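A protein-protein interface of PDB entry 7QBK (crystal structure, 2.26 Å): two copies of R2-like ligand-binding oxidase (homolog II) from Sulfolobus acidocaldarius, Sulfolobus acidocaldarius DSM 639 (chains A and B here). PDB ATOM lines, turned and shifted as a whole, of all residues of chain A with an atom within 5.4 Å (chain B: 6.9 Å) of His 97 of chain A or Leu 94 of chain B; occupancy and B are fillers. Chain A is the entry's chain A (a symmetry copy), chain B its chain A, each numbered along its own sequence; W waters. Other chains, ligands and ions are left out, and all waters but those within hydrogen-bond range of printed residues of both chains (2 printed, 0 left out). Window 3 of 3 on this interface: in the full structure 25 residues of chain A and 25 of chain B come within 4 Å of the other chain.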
ATOM      1  N   ALA A  93       0.279 -20.897  18.228  1.00  0.00           N
ATOM      2  CA  ALA A  93      -0.637 -19.763  18.232  1.00  0.00           C
ATOM      3  C   ALA A  93      -1.149 -19.459  19.635  1.00  0.00           C
ATOM      4  O   ALA A  93      -1.331 -18.288  19.987  1.00  0.00           O
ATOM      5  CB  ALA A  93      -1.804 -20.031  17.282  1.00  0.00           C
ATOM      6  N   LEU A  94      -1.362 -20.491  20.454  1.00  0.00           N
ATOM      7  CA  LEU A  94      -1.900 -20.321  21.799  1.00  0.00           C
ATOM      8  C   LEU A  94      -0.814 -20.036  22.834  1.00  0.00           C
ATOM      9  O   LEU A  94      -0.957 -19.123  23.651  1.00  0.00           O
ATOM     10  CB  LEU A  94      -2.701 -21.563  22.202  1.00  0.00           C
ATOM     11  CG  LEU A  94      -3.971 -21.838  21.392  1.00  0.00           C
ATOM     12  CD1 LEU A  94      -4.586 -23.161  21.808  1.00  0.00           C
ATOM     13  CD2 LEU A  94      -4.975 -20.699  21.551  1.00  0.00           C
ATOM     14  N   ASP A  95       0.279 -20.799  22.812  1.00  0.00           N
ATOM     15  CA  ASP A  95       1.307 -20.626  23.830  1.00  0.00           C
ATOM     16  C   ASP A  95       2.133 -19.359  23.648  1.00  0.00           C
ATOM     17  O   ASP A  95       2.934 -19.039  24.530  1.00  0.00           O
ATOM     18  CB  ASP A  95       2.226 -21.847  23.855  1.00  0.00           C
ATOM     19  CG  ASP A  95       1.492 -23.112  24.235  1.00  0.00           C
ATOM     20  OD1 ASP A  95       0.482 -23.003  24.962  1.00  0.00           O
ATOM     21  OD2 ASP A  95       1.912 -24.207  23.807  1.00  0.00           O
ATOM     22  N   LEU A  96       1.965 -18.626  22.549  1.00  0.00           N
ATOM     23  CA  LEU A  96       2.760 -17.419  22.354  1.00  0.00           C
ATOM     24  C   LEU A  96       2.197 -16.205  23.082  1.00  0.00           C
ATOM     25  O   LEU A  96       2.786 -15.123  22.990  1.00  0.00           O
ATOM     26  CB  LEU A  96       2.892 -17.099  20.867  1.00  0.00           C
ATOM     27  CG  LEU A  96       4.330 -16.872  20.413  1.00  0.00           C
ATOM     28  CD1 LEU A  96       5.054 -18.203  20.325  1.00  0.00           C
ATOM     29  CD2 LEU A  96       4.368 -16.140  19.090  1.00  0.00           C
ATOM     30  N   HIS A  97       1.084 -16.360  23.795  1.00  0.00           N
ATOM     31  CA  HIS A  97       0.501 -15.243  24.534  1.00  0.00           C
ATOM     32  C   HIS A  97       1.450 -14.598  25.546  1.00  0.00           C
ATOM     33  O   HIS A  97       1.449 -13.358  25.637  1.00  0.00           O
ATOM     34  CB  HIS A  97      -0.790 -15.718  25.215  1.00  0.00           C
ATOM     35  CG  HIS A  97      -1.464 -14.667  26.041  1.00  0.00           C
ATOM     36  ND1 HIS A  97      -2.286 -13.704  25.495  1.00  0.00           N
ATOM     37  CD2 HIS A  97      -1.447 -14.435  27.375  1.00  0.00           C
ATOM     38  CE1 HIS A  97      -2.739 -12.921  26.456  1.00  0.00           C
ATOM     39  NE2 HIS A  97      -2.246 -13.342  27.606  1.00  0.00           N
ATOM     40  N   PRO A  98       2.249 -15.333  26.333  1.00  0.00           N
ATOM     41  CA  PRO A  98       3.106 -14.642  27.316  1.00  0.00           C
ATOM     42  C   PRO A  98       4.167 -13.755  26.690  1.00  0.00           C
ATOM     43  O   PRO A  98       4.491 -12.705  27.256  1.00  0.00           O
ATOM     44  CB  PRO A  98       3.734 -15.799  28.106  1.00  0.00           C
ATOM     45  CG  PRO A  98       2.814 -16.931  27.925  1.00  0.00           C
ATOM     46  CD  PRO A  98       2.277 -16.794  26.538  1.00  0.00           C
ATOM     47  N   LEU A  99       4.731 -14.152  25.546  1.00  0.00           N
ATOM     48  CA  LEU A  99       5.753 -13.324  24.910  1.00  0.00           C
ATOM     49  C   LEU A  99       5.178 -11.981  24.474  1.00  0.00           C
ATOM     50  O   LEU A  99       5.813 -10.935  24.657  1.00  0.00           O
ATOM     51  CB  LEU A  99       6.361 -14.061  23.715  1.00  0.00           C
ATOM     52  CG  LEU A  99       7.539 -13.395  23.001  1.00  0.00           C
ATOM     53  CD1 LEU A  99       8.706 -13.224  23.952  1.00  0.00           C
ATOM     54  CD2 LEU A  99       7.955 -14.206  21.787  1.00  0.00           C
ATOM     55  N   ILE A 100       3.974 -11.991  23.899  1.00  0.00           N
ATOM     56  CA  ILE A 100       3.358 -10.749  23.446  1.00  0.00           C
ATOM     57  C   ILE A 100       3.035  -9.852  24.632  1.00  0.00           C
ATOM     58  O   ILE A 100       3.247  -8.635  24.581  1.00  0.00           O
ATOM     59  CB  ILE A 100       2.106 -11.047  22.601  1.00  0.00           C
ATOM     60  CG1 ILE A 100       2.440 -12.014  21.462  1.00  0.00           C
ATOM     61  CG2 ILE A 100       1.515  -9.756  22.060  1.00  0.00           C
ATOM     62  CD1 ILE A 100       1.243 -12.412  20.614  1.00  0.00           C
ATOM     63  N   VAL A 101       2.518 -10.435  25.718  1.00  0.00           N
ATOM     64  CA  VAL A 101       2.253  -9.662  26.929  1.00  0.00           C
ATOM     65  C   VAL A 101       3.552  -9.101  27.498  1.00  0.00           C
ATOM     66  O   VAL A 101       3.602  -7.956  27.958  1.00  0.00           O
ATOM     67  CB  VAL A 101       1.503 -10.524  27.964  1.00  0.00           C
ATOM     68  CG1 VAL A 101       1.304  -9.757  29.263  1.00  0.00           C
ATOM     69  CG2 VAL A 101       0.164 -10.980  27.408  1.00  0.00           C
ATOM     70  N   THR A 102       4.627  -9.892  27.464  1.00  0.00           N
ATOM     71  CA  THR A 102       5.920  -9.403  27.939  1.00  0.00           C
ATOM     72  C   THR A 102       6.369  -8.183  27.149  1.00  0.00           C
ATOM     73  O   THR A 102       6.788  -7.173  27.727  1.00  0.00           O
ATOM     74  CB  THR A 102       6.979 -10.506  27.849  1.00  0.00           C
ATOM     75  OG1 THR A 102       6.622 -11.596  28.706  1.00  0.00           O
ATOM     76  CG2 THR A 102       8.344  -9.965  28.264  1.00  0.00           C
ATOM     77  N   VAL A 104       4.657  -6.033  25.325  1.00  0.00           N
ATOM     78  CA  VAL A 104       3.828  -4.836  25.452  1.00  0.00           C
ATOM     79  C   VAL A 104       4.080  -4.145  26.789  1.00  0.00           C
ATOM     80  O   VAL A 104       4.005  -2.912  26.877  1.00  0.00           O
ATOM     81  CB  VAL A 104       2.336  -5.174  25.245  1.00  0.00           C
ATOM     82  CG1 VAL A 104       1.798  -6.030  26.374  1.00  0.00           C
ATOM     83  CG2 VAL A 104       1.514  -3.901  25.106  1.00  0.00           C
ATOM     84  N   MET A 165       7.441 -20.892  27.361  1.00  0.00           N
ATOM     85  CA  MET A 165       6.595 -19.724  27.139  1.00  0.00           C
ATOM     86  C   MET A 165       5.956 -19.249  28.435  1.00  0.00           C
ATOM     87  O   MET A 165       6.021 -18.061  28.772  1.00  0.00           O
ATOM     88  CB  MET A 165       5.524 -20.038  26.095  1.00  0.00           C
ATOM     89  CG  MET A 165       6.064 -20.287  24.688  1.00  0.00           C
ATOM     90  SD  MET A 165       6.970 -18.885  23.989  1.00  0.00           S
ATOM     91  CE  MET A 165       5.821 -17.552  24.313  1.00  0.00           C
ATOM     92  N   TRP A 166       5.339 -20.157  29.180  1.00  0.00           N
ATOM     93  CA  TRP A 166       4.700 -19.765  30.426  1.00  0.00           C
ATOM     94  C   TRP A 166       5.698 -19.529  31.555  1.00  0.00           C
ATOM     95  O   TRP A 166       5.289 -19.121  32.647  1.00  0.00           O
ATOM     96  CB  TRP A 166       3.648 -20.807  30.814  1.00  0.00           C
ATOM     97  CG  TRP A 166       2.540 -20.898  29.789  1.00  0.00           C
ATOM     98  CD1 TRP A 166       2.379 -21.861  28.835  1.00  0.00           C
ATOM     99  CD2 TRP A 166       1.463 -19.967  29.601  1.00  0.00           C
ATOM    100  NE1 TRP A 166       1.266 -21.597  28.075  1.00  0.00           N
ATOM    101  CE2 TRP A 166       0.686 -20.440  28.524  1.00  0.00           C
ATOM    102  CE3 TRP A 166       1.078 -18.787  30.245  1.00  0.00           C
ATOM    103  CZ2 TRP A 166      -0.455 -19.773  28.076  1.00  0.00           C
ATOM    104  CZ3 TRP A 166      -0.055 -18.125  29.798  1.00  0.00           C
ATOM    105  CH2 TRP A 166      -0.808 -18.622  28.725  1.00  0.00           C
ATOM    106  N   GLY B  88      -8.420  -0.143  24.599  1.00  0.00           N
ATOM    107  CA  GLY B  88      -9.512  -1.083  24.803  1.00  0.00           C
ATOM    108  C   GLY B  88      -9.449  -2.264  23.853  1.00  0.00           C
ATOM    109  O   GLY B  88      -9.547  -3.419  24.275  1.00  0.00           O
ATOM    110  N   GLU B  89      -9.283  -1.989  22.552  1.00  0.00           N
ATOM    111  CA  GLU B  89      -9.155  -3.062  21.569  1.00  0.00           C
ATOM    112  C   GLU B  89      -7.949  -3.949  21.866  1.00  0.00           C
ATOM    113  O   GLU B  89      -7.991  -5.160  21.619  1.00  0.00           O
ATOM    114  CB  GLU B  89      -9.038  -2.480  20.156  1.00  0.00           C
ATOM    115  CG  GLU B  89     -10.147  -1.517  19.742  1.00  0.00           C
ATOM    116  CD  GLU B  89     -11.257  -2.187  18.959  1.00  0.00           C
ATOM    117  OE1 GLU B  89     -11.154  -3.402  18.724  1.00  0.00           O
ATOM    118  OE2 GLU B  89     -12.227  -1.502  18.571  1.00  0.00           O
ATOM    119  N   GLU B  90      -6.867  -3.369  22.391  1.00  0.00           N
ATOM    120  CA  GLU B  90      -5.717  -4.183  22.760  1.00  0.00           C
ATOM    121  C   GLU B  90      -6.027  -5.040  23.979  1.00  0.00           C
ATOM    122  O   GLU B  90      -5.624  -6.208  24.041  1.00  0.00           O
ATOM    123  CB  GLU B  90      -4.501  -3.296  23.010  1.00  0.00           C
ATOM    124  CG  GLU B  90      -3.259  -4.061  23.433  1.00  0.00           C
ATOM    125  CD  GLU B  90      -2.001  -3.227  23.319  1.00  0.00           C
ATOM    126  OE1 GLU B  90      -1.521  -3.027  22.182  1.00  0.00           O
ATOM    127  OE2 GLU B  90      -1.502  -2.757  24.363  1.00  0.00           O
ATOM    128  N   ALA B  91      -6.756  -4.482  24.953  1.00  0.00           N
ATOM    129  CA  ALA B  91      -7.152  -5.264  26.120  1.00  0.00           C
ATOM    130  C   ALA B  91      -8.026  -6.445  25.722  1.00  0.00           C
ATOM    131  O   ALA B  91      -7.880  -7.545  26.266  1.00  0.00           O
ATOM    132  CB  ALA B  91      -7.880  -4.374  27.127  1.00  0.00           C
ATOM    133  N   VAL B  92      -8.941  -6.242  24.773  1.00  0.00           N
ATOM    134  CA  VAL B  92      -9.789  -7.342  24.327  1.00  0.00           C
ATOM    135  C   VAL B  92      -8.964  -8.387  23.589  1.00  0.00           C
ATOM    136  O   VAL B  92      -9.123  -9.592  23.814  1.00  0.00           O
ATOM    137  CB  VAL B  92     -10.945  -6.811  23.459  1.00  0.00           C
ATOM    138  CG1 VAL B  92     -11.788  -7.961  22.931  1.00  0.00           C
ATOM    139  CG2 VAL B  92     -11.806  -5.869  24.276  1.00  0.00           C
ATOM    140  N   ALA B  93      -8.064  -7.945  22.708  1.00  0.00           N
ATOM    141  CA  ALA B  93      -7.264  -8.888  21.936  1.00  0.00           C
ATOM    142  C   ALA B  93      -6.401  -9.762  22.837  1.00  0.00           C
ATOM    143  O   ALA B  93      -6.210 -10.949  22.548  1.00  0.00           O
ATOM    144  CB  ALA B  93      -6.394  -8.135  20.930  1.00  0.00           C
ATOM    145  N   LEU B  94      -5.896  -9.208  23.940  1.00  0.00           N
ATOM    146  CA  LEU B  94      -5.014  -9.936  24.847  1.00  0.00           C
ATOM    147  C   LEU B  94      -5.784 -10.736  25.896  1.00  0.00           C
ATOM    148  O   LEU B  94      -5.481 -11.910  26.128  1.00  0.00           O
ATOM    149  CB  LEU B  94      -4.049  -8.963  25.530  1.00  0.00           C
ATOM    150  CG  LEU B  94      -3.041  -8.261  24.615  1.00  0.00           C
ATOM    151  CD1 LEU B  94      -2.243  -7.235  25.399  1.00  0.00           C
ATOM    152  CD2 LEU B  94      -2.115  -9.272  23.948  1.00  0.00           C
ATOM    153  N   ASP B  95      -6.783 -10.126  26.532  1.00  0.00           N
ATOM    154  CA  ASP B  95      -7.494 -10.816  27.601  1.00  0.00           C
ATOM    155  C   ASP B  95      -8.424 -11.913  27.099  1.00  0.00           C
ATOM    156  O   ASP B  95      -8.965 -12.657  27.922  1.00  0.00           O
ATOM    157  CB  ASP B  95      -8.282  -9.809  28.438  1.00  0.00           C
ATOM    158  CG  ASP B  95      -7.383  -8.811  29.131  1.00  0.00           C
ATOM    159  OD1 ASP B  95      -6.222  -9.169  29.411  1.00  0.00           O
ATOM    160  OD2 ASP B  95      -7.831  -7.672  29.388  1.00  0.00           O
ATOM    161  N   LEU B  96      -8.622 -12.049  25.790  1.00  0.00           N
ATOM    162  CA  LEU B  96      -9.522 -13.086  25.297  1.00  0.00           C
ATOM    163  C   LEU B  96      -8.863 -14.457  25.199  1.00  0.00           C
ATOM    164  O   LEU B  96      -9.528 -15.414  24.792  1.00  0.00           O
ATOM    165  CB  LEU B  96     -10.088 -12.700  23.933  1.00  0.00           C
ATOM    166  CG  LEU B  96     -11.609 -12.794  23.849  1.00  0.00           C
ATOM    167  CD1 LEU B  96     -12.232 -11.623  24.587  1.00  0.00           C
ATOM    168  CD2 LEU B  96     -12.067 -12.841  22.408  1.00  0.00           C
ATOM    169  N   HIS B  97      -7.587 -14.568  25.559  1.00  0.00           N
ATOM    170  CA  HIS B  97      -6.900 -15.855  25.508  1.00  0.00           C
ATOM    171  C   HIS B  97      -7.569 -16.956  26.334  1.00  0.00           C
ATOM    172  O   HIS B  97      -7.629 -18.097  25.844  1.00  0.00           O
ATOM    173  CB  HIS B  97      -5.440 -15.656  25.938  1.00  0.00           C
ATOM    174  CG  HIS B  97      -4.634 -16.917  25.966  1.00  0.00           C
ATOM    175  ND1 HIS B  97      -4.069 -17.465  24.835  1.00  0.00           N
ATOM    176  CD2 HIS B  97      -4.293 -17.734  26.990  1.00  0.00           C
ATOM    177  CE1 HIS B  97      -3.420 -18.568  25.160  1.00  0.00           C
ATOM    178  NE2 HIS B  97      -3.539 -18.754  26.461  1.00  0.00           N
ATOM    179  N   PRO B  98      -8.062 -16.718  27.559  1.00  0.00           N
ATOM    180  CA  PRO B  98      -8.654 -17.840  28.313  1.00  0.00           C
ATOM    181  C   PRO B  98      -9.907 -18.414  27.677  1.00  0.00           C
ATOM    182  O   PRO B  98     -10.132 -19.627  27.766  1.00  0.00           O
ATOM    183  CB  PRO B  98      -8.953 -17.220  29.685  1.00  0.00           C
ATOM    184  CG  PRO B  98      -8.045 -16.069  29.791  1.00  0.00           C
ATOM    185  CD  PRO B  98      -7.929 -15.520  28.407  1.00  0.00           C
ATOM    186  N   ILE B 119      -9.902 -12.327  17.234  1.00  0.00           N
ATOM    187  CA  ILE B 119      -8.718 -11.753  17.867  1.00  0.00           C
ATOM    188  C   ILE B 119      -7.898 -10.957  16.864  1.00  0.00           C
ATOM    189  O   ILE B 119      -7.423  -9.856  17.169  1.00  0.00           O
ATOM    190  CB  ILE B 119      -7.885 -12.862  18.535  1.00  0.00           C
ATOM    191  CG1 ILE B 119      -8.557 -13.290  19.829  1.00  0.00           C
ATOM    192  CG2 ILE B 119      -6.477 -12.379  18.814  1.00  0.00           C
ATOM    193  CD1 ILE B 119      -8.857 -12.127  20.729  1.00  0.00           C
ATOM    194  N   GLU B 122      -9.518  -7.654  16.091  1.00  0.00           N
ATOM    195  CA  GLU B 122      -9.279  -6.724  17.191  1.00  0.00           C
ATOM    196  C   GLU B 122      -7.895  -6.098  17.096  1.00  0.00           C
ATOM    197  O   GLU B 122      -7.746  -4.879  17.233  1.00  0.00           O
ATOM    198  CB  GLU B 122      -9.451  -7.431  18.538  1.00  0.00           C
ATOM    199  CG  GLU B 122     -10.880  -7.850  18.845  1.00  0.00           C
ATOM    200  CD  GLU B 122     -11.846  -6.684  18.834  1.00  0.00           C
ATOM    201  OE1 GLU B 122     -11.411  -5.555  19.124  1.00  0.00           O
ATOM    202  OE2 GLU B 122     -13.039  -6.890  18.537  1.00  0.00           O
ATOM    203  N   TRP B 166      -9.884 -13.957  33.034  1.00  0.00           N
ATOM    204  CA  TRP B 166      -8.951 -14.831  33.726  1.00  0.00           C
ATOM    205  C   TRP B 166      -9.606 -15.625  34.851  1.00  0.00           C
ATOM    206  O   TRP B 166      -8.935 -16.458  35.472  1.00  0.00           O
ATOM    207  CB  TRP B 166      -7.763 -14.010  34.235  1.00  0.00           C
ATOM    208  CG  TRP B 166      -6.984 -13.385  33.101  1.00  0.00           C
ATOM    209  CD1 TRP B 166      -7.029 -12.083  32.691  1.00  0.00           C
ATOM    210  CD2 TRP B 166      -6.070 -14.048  32.215  1.00  0.00           C
ATOM    211  NE1 TRP B 166      -6.195 -11.893  31.615  1.00  0.00           N
ATOM    212  CE2 TRP B 166      -5.594 -13.084  31.303  1.00  0.00           C
ATOM    213  CE3 TRP B 166      -5.602 -15.363  32.110  1.00  0.00           C
ATOM    214  CZ2 TRP B 166      -4.675 -13.391  30.300  1.00  0.00           C
ATOM    215  CZ3 TRP B 166      -4.690 -15.666  31.112  1.00  0.00           C
ATOM    216  CH2 TRP B 166      -4.235 -14.684  30.222  1.00  0.00           C
HETATM  217  O   HOH W   1      -5.036 -13.280  23.597  1.00  0.00           O
HETATM  218  O   HOH W   2      -1.999 -16.783  22.266  1.00  0.00           O
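Hydrophobic or aromatic side chains of chain A that line the printed part of chain B: His 97, Val 104 and Trp 166.
Along chain A the printed residues that touch a printed residue of chain B span positions 94 to 166.
Along chain B the printed residues that touch a printed residue of chain A span positions 90 to 166.
Among the printed residues, no Asp or Glu carboxylate lies within 4 Å of a Lys or Arg side-chain nitrogen of the other chain.
Of the printed residues of chain B, Leu 94 of chain A touches His 97 (2.9 Å).
Of the printed residues of chain A, Glu 90 of chain B touches Val 104 (3.3 Å).
Leu 94 of chain B touches just one residue of chain A: His 97.
Water W2 lies within hydrogen-bond range of the backbone carbonyl oxygen (O) of Ala 93 of chain A (2.8 Å), the backbone carbonyl oxygen (O) of Leu 94 of chain A (2.9 Å), a ring nitrogen (ND1) of His 97 of chain B (3.4 Å) and the backbone NH (N) of His 97 of chain A (3.5 Å).
Water W1 lies within hydrogen-bond range of O of Ala 93 of chain B (2.8 Å), O of Leu 94 of chain B (2.9 Å), ND1 of His 97 of chain A (3.4 Å) and N of His 97 of chain B (3.5 Å).
Leu 94 of chain A touches His 97 of chain B, and with the chains exchanged His 97 of chain A touches Leu 94 of chain B.
His 97 of chain A touches its own counterpart, His 97 of chain B.
His 97 of chain A touches Trp 166 of chain B, and with the chains exchanged Trp 166 of chain A touches His 97 of chain B.
7 positions are printed for both chains.
Of the 6 pairs that touch across the chains among the printed residues, 5 have their exchanged pair printed and touching as well.
O of Leu 94 of chain A touches CE1 of His 97 of chain B (2.9 Å).
CE1 of His 97 of chain A touches O of Leu 94 of chain B, at 2.9 Å.
His 97 of chain B touches His 97 of chain A (ND1 to CB, 3.7 Å).
Trp 166 of chain B touches His 97 of chain A (CH2 to NE2, 3.5 Å).
Glu 90 of chain B touches Val 104 of chain A.
Trp 166 of chain A touches His 97 of chain B (CH2 to NE2, 3.5 Å).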
